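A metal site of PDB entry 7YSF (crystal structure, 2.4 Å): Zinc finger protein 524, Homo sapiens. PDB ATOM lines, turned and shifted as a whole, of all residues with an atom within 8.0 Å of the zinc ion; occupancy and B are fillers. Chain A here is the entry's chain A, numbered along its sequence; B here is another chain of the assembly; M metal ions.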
ATOM      1  N   GLN A  39     -17.116 -14.443 -12.441  1.00  0.00           N
ATOM      2  CA  GLN A  39     -16.081 -13.424 -12.460  1.00  0.00           C
ATOM      3  C   GLN A  39     -16.202 -12.623 -13.753  1.00  0.00           C
ATOM      4  O   GLN A  39     -16.284 -13.200 -14.841  1.00  0.00           O
ATOM      5  CB  GLN A  39     -14.683 -14.041 -12.356  1.00  0.00           C
ATOM      6  CG  GLN A  39     -13.539 -13.032 -12.501  1.00  0.00           C
ATOM      7  CD  GLN A  39     -12.179 -13.638 -12.214  1.00  0.00           C
ATOM      8  OE1 GLN A  39     -11.848 -14.728 -12.689  1.00  0.00           O
ATOM      9  NE2 GLN A  39     -11.375 -12.934 -11.431  1.00  0.00           N
ATOM     10  N   CYS A  40     -16.226 -11.295 -13.620  1.00  0.00           N
ATOM     11  CA  CYS A  40     -16.174 -10.398 -14.768  1.00  0.00           C
ATOM     12  C   CYS A  40     -14.739 -10.311 -15.273  1.00  0.00           C
ATOM     13  O   CYS A  40     -13.859  -9.816 -14.560  1.00  0.00           O
ATOM     14  CB  CYS A  40     -16.694  -9.020 -14.358  1.00  0.00           C
ATOM     15  SG  CYS A  40     -16.504  -7.712 -15.600  1.00  0.00           S
ATOM     16  N   LYS A  41     -14.504 -10.759 -16.502  1.00  0.00           N
ATOM     17  CA  LYS A  41     -13.156 -10.734 -17.040  1.00  0.00           C
ATOM     18  C   LYS A  41     -12.737  -9.350 -17.535  1.00  0.00           C
ATOM     19  O   LYS A  41     -11.637  -9.228 -18.089  1.00  0.00           O
ATOM     20  CB  LYS A  41     -13.006 -11.760 -18.175  1.00  0.00           C
ATOM     21  CG  LYS A  41     -13.390 -13.181 -17.751  1.00  0.00           C
ATOM     22  CD  LYS A  41     -12.150 -14.031 -17.482  1.00  0.00           C
ATOM     23  CE  LYS A  41     -12.433 -15.066 -16.414  1.00  0.00           C
ATOM     24  NZ  LYS A  41     -11.934 -16.404 -16.789  1.00  0.00           N
ATOM     25  N   VAL A  42     -13.579  -8.332 -17.369  1.00  0.00           N
ATOM     26  CA  VAL A  42     -13.188  -6.957 -17.662  1.00  0.00           C
ATOM     27  C   VAL A  42     -12.417  -6.345 -16.501  1.00  0.00           C
ATOM     28  O   VAL A  42     -11.325  -5.792 -16.688  1.00  0.00           O
ATOM     29  CB  VAL A  42     -14.444  -6.120 -18.011  1.00  0.00           C
ATOM     30  CG1 VAL A  42     -14.079  -4.649 -18.116  1.00  0.00           C
ATOM     31  CG2 VAL A  42     -15.093  -6.627 -19.280  1.00  0.00           C
ATOM     32  N   CYS A  43     -12.969  -6.408 -15.292  1.00  0.00           N
ATOM     33  CA  CYS A  43     -12.361  -5.788 -14.128  1.00  0.00           C
ATOM     34  C   CYS A  43     -11.909  -6.767 -13.052  1.00  0.00           C
ATOM     35  O   CYS A  43     -11.128  -6.374 -12.178  1.00  0.00           O
ATOM     36  CB  CYS A  43     -13.323  -4.772 -13.492  1.00  0.00           C
ATOM     37  SG  CYS A  43     -14.750  -5.513 -12.655  1.00  0.00           S
ATOM     38  N   GLY A  44     -12.382  -8.011 -13.083  1.00  0.00           N
ATOM     39  CA  GLY A  44     -11.924  -9.048 -12.175  1.00  0.00           C
ATOM     40  C   GLY A  44     -12.857  -9.359 -11.021  1.00  0.00           C
ATOM     41  O   GLY A  44     -12.698 -10.398 -10.384  1.00  0.00           O
ATOM     42  N   LYS A  45     -13.818  -8.482 -10.738  1.00  0.00           N
ATOM     43  CA  LYS A  45     -14.689  -8.682  -9.580  1.00  0.00           C
ATOM     44  C   LYS A  45     -15.528  -9.940  -9.739  1.00  0.00           C
ATOM     45  O   LYS A  45     -15.988 -10.276 -10.828  1.00  0.00           O
ATOM     46  CB  LYS A  45     -15.584  -7.467  -9.382  1.00  0.00           C
ATOM     47  CG  LYS A  45     -14.840  -6.197  -8.980  1.00  0.00           C
ATOM     48  CD  LYS A  45     -15.704  -4.963  -9.189  1.00  0.00           C
ATOM     49  CE  LYS A  45     -15.026  -3.717  -8.625  1.00  0.00           C
ATOM     50  NZ  LYS A  45     -15.536  -3.385  -7.264  1.00  0.00           N
ATOM     51  N   THR A  46     -15.729 -10.640  -8.616  1.00  0.00           N
ATOM     52  CA  THR A  46     -16.507 -11.863  -8.590  1.00  0.00           C
ATOM     53  C   THR A  46     -17.900 -11.600  -8.040  1.00  0.00           C
ATOM     54  O   THR A  46     -18.136 -10.621  -7.318  1.00  0.00           O
ATOM     55  CB  THR A  46     -15.810 -12.946  -7.747  1.00  0.00           C
ATOM     56  OG1 THR A  46     -15.848 -12.572  -6.361  1.00  0.00           O
ATOM     57  CG2 THR A  46     -14.361 -13.117  -8.186  1.00  0.00           C
ATOM     58  N   PHE A  47     -18.827 -12.486  -8.383  1.00  0.00           N
ATOM     59  CA  PHE A  47     -20.236 -12.285  -8.054  1.00  0.00           C
ATOM     60  C   PHE A  47     -20.887 -13.602  -7.659  1.00  0.00           C
ATOM     61  O   PHE A  47     -20.460 -14.678  -8.078  1.00  0.00           O
ATOM     62  CB  PHE A  47     -20.989 -11.647  -9.231  1.00  0.00           C
ATOM     63  CG  PHE A  47     -20.502 -10.273  -9.559  1.00  0.00           C
ATOM     64  CD1 PHE A  47     -21.022  -9.158  -8.915  1.00  0.00           C
ATOM     65  CD2 PHE A  47     -19.489 -10.088 -10.488  1.00  0.00           C
ATOM     66  CE1 PHE A  47     -20.555  -7.899  -9.199  1.00  0.00           C
ATOM     67  CE2 PHE A  47     -19.014  -8.830 -10.777  1.00  0.00           C
ATOM     68  CZ  PHE A  47     -19.551  -7.728 -10.122  1.00  0.00           C
ATOM     69  N   LEU A  53     -23.721 -10.677 -12.030  1.00  0.00           N
ATOM     70  CA  LEU A  53     -22.677 -10.443 -13.032  1.00  0.00           C
ATOM     71  C   LEU A  53     -23.236  -9.720 -14.253  1.00  0.00           C
ATOM     72  O   LEU A  53     -22.620  -8.780 -14.755  1.00  0.00           O
ATOM     73  CB  LEU A  53     -22.045 -11.777 -13.440  1.00  0.00           C
ATOM     74  CG  LEU A  53     -21.057 -11.683 -14.601  1.00  0.00           C
ATOM     75  CD1 LEU A  53     -19.834 -10.863 -14.191  1.00  0.00           C
ATOM     76  CD2 LEU A  53     -20.644 -13.069 -15.085  1.00  0.00           C
ATOM     77  N   HIS A  56     -23.897  -6.213 -13.412  1.00  0.00           N
ATOM     78  CA  HIS A  56     -22.630  -5.507 -13.291  1.00  0.00           C
ATOM     79  C   HIS A  56     -21.984  -5.256 -14.646  1.00  0.00           C
ATOM     80  O   HIS A  56     -21.308  -4.234 -14.839  1.00  0.00           O
ATOM     81  CB  HIS A  56     -21.676  -6.286 -12.393  1.00  0.00           C
ATOM     82  CG  HIS A  56     -20.233  -5.905 -12.559  1.00  0.00           C
ATOM     83  ND1 HIS A  56     -19.618  -4.958 -11.779  1.00  0.00           N
ATOM     84  CD2 HIS A  56     -19.294  -6.351 -13.422  1.00  0.00           C
ATOM     85  CE1 HIS A  56     -18.356  -4.828 -12.151  1.00  0.00           C
ATOM     86  NE2 HIS A  56     -18.135  -5.668 -13.148  1.00  0.00           N
ATOM     87  N   CYS A  57     -22.171  -6.170 -15.599  1.00  0.00           N
ATOM     88  CA  CYS A  57     -21.587  -5.998 -16.926  1.00  0.00           C
ATOM     89  C   CYS A  57     -22.092  -4.717 -17.592  1.00  0.00           C
ATOM     90  O   CYS A  57     -21.382  -4.130 -18.411  1.00  0.00           O
ATOM     91  CB  CYS A  57     -21.922  -7.211 -17.801  1.00  0.00           C
ATOM     92  SG  CYS A  57     -20.692  -7.601 -19.079  1.00  0.00           S
ATOM     93  N   ASN A  58     -23.315  -4.290 -17.251  1.00  0.00           N
ATOM     94  CA  ASN A  58     -23.857  -3.077 -17.831  1.00  0.00           C
ATOM     95  C   ASN A  58     -23.039  -1.841 -17.457  1.00  0.00           C
ATOM     96  O   ASN A  58     -23.022  -0.864 -18.202  1.00  0.00           O
ATOM     97  CB  ASN A  58     -25.317  -2.885 -17.395  1.00  0.00           C
ATOM     98  CG  ASN A  58     -26.227  -3.973 -17.921  1.00  0.00           C
ATOM     99  OD1 ASN A  58     -25.998  -4.535 -18.990  1.00  0.00           O
ATOM    100  ND2 ASN A  58     -27.296  -4.264 -17.176  1.00  0.00           N
ATOM    101  N   ILE A  59     -22.363  -1.879 -16.299  1.00  0.00           N
ATOM    102  CA  ILE A  59     -21.610  -0.719 -15.845  1.00  0.00           C
ATOM    103  C   ILE A  59     -20.508  -0.366 -16.832  1.00  0.00           C
ATOM    104  O   ILE A  59     -20.268   0.810 -17.142  1.00  0.00           O
ATOM    105  CB  ILE A  59     -21.036  -0.978 -14.433  1.00  0.00           C
ATOM    106  CG1 ILE A  59     -22.165  -0.984 -13.399  1.00  0.00           C
ATOM    107  CG2 ILE A  59     -20.008   0.068 -14.071  1.00  0.00           C
ATOM    108  CD1 ILE A  59     -21.806  -1.676 -12.104  1.00  0.00           C
ATOM    109  N   HIS A  60     -19.825  -1.381 -17.383  1.00  0.00           N
ATOM    110  CA  HIS A  60     -18.705  -1.156 -18.282  1.00  0.00           C
ATOM    111  C   HIS A  60     -19.115  -0.551 -19.623  1.00  0.00           C
ATOM    112  O   HIS A  60     -18.237  -0.228 -20.433  1.00  0.00           O
ATOM    113  CB  HIS A  60     -17.946  -2.460 -18.513  1.00  0.00           C
ATOM    114  CG  HIS A  60     -17.311  -3.007 -17.275  1.00  0.00           C
ATOM    115  ND1 HIS A  60     -16.561  -2.230 -16.420  1.00  0.00           N
ATOM    116  CD2 HIS A  60     -17.312  -4.246 -16.743  1.00  0.00           C
ATOM    117  CE1 HIS A  60     -16.130  -2.966 -15.419  1.00  0.00           C
ATOM    118  NE2 HIS A  60     -16.570  -4.196 -15.590  1.00  0.00           N
ATOM    119  P    DG B   8     -20.395  -4.212  -8.328  1.00  0.00           P
ATOM    120  OP1  DG B   8     -19.023  -4.761  -8.353  1.00  0.00           O
ATOM    121  OP2  DG B   8     -21.173  -4.127  -9.583  1.00  0.00           O
ATOM    122  O5'  DG B   8     -21.225  -5.032  -7.244  1.00  0.00           O
ATOM    123  C5'  DG B   8     -20.723  -5.103  -5.923  1.00  0.00           C
ATOM    124  C4'  DG B   8     -21.806  -5.479  -4.939  1.00  0.00           C
ATOM    125  O4'  DG B   8     -22.938  -4.589  -5.101  1.00  0.00           O
ATOM    126  C3'  DG B   8     -22.359  -6.891  -5.070  1.00  0.00           C
ATOM    127  O3'  DG B   8     -22.217  -7.562  -3.822  1.00  0.00           O
ATOM    128  C2'  DG B   8     -23.839  -6.685  -5.442  1.00  0.00           C
ATOM    129  C1'  DG B   8     -24.104  -5.323  -4.832  1.00  0.00           C
ATOM    130  N9   DG B   8     -25.230  -4.599  -5.408  1.00  0.00           N
ATOM    131  C8   DG B   8     -25.368  -4.153  -6.704  1.00  0.00           C
ATOM    132  N7   DG B   8     -26.489  -3.502  -6.901  1.00  0.00           N
ATOM    133  C5   DG B   8     -27.110  -3.508  -5.661  1.00  0.00           C
ATOM    134  C6   DG B   8     -28.363  -2.960  -5.258  1.00  0.00           C
ATOM    135  O6   DG B   8     -29.181  -2.340  -5.948  1.00  0.00           O
ATOM    136  N1   DG B   8     -28.620  -3.196  -3.908  1.00  0.00           N
ATOM    137  C2   DG B   8     -27.781  -3.875  -3.060  1.00  0.00           C
ATOM    138  N2   DG B   8     -28.205  -4.002  -1.787  1.00  0.00           N
ATOM    139  N3   DG B   8     -26.615  -4.393  -3.418  1.00  0.00           N
ATOM    140  C4   DG B   8     -26.349  -4.175  -4.731  1.00  0.00           C
HETATM  141 ZN    ZN M   1     -16.408  -5.818 -14.318  1.00  0.00          ZN
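ND1 of His 56 lies within hydrogen-bond range of OP2 of DG 8 of chain B (2.8 Å).
SG of Cys 40 lies close to N of Val 42 (3.5 Å).
The backbone carbonyl oxygen (O) of Lys 45 lies within hydrogen-bond range of the backbone NH (N) of Cys 40 (3.0 Å).
The backbone NH (N) of Lys 45 sits close to the side-chain sulfur (SG) of Cys 43, at 3.7 Å.
The zinc ion is bound by NE2 of His 60 (2.1 Å), NE2 of His 56 (2.1 Å), SG of Cys 40 (2.3 Å) and SG of Cys 43 (2.4 Å).
The zinc ion has four donor atoms within binding distance.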
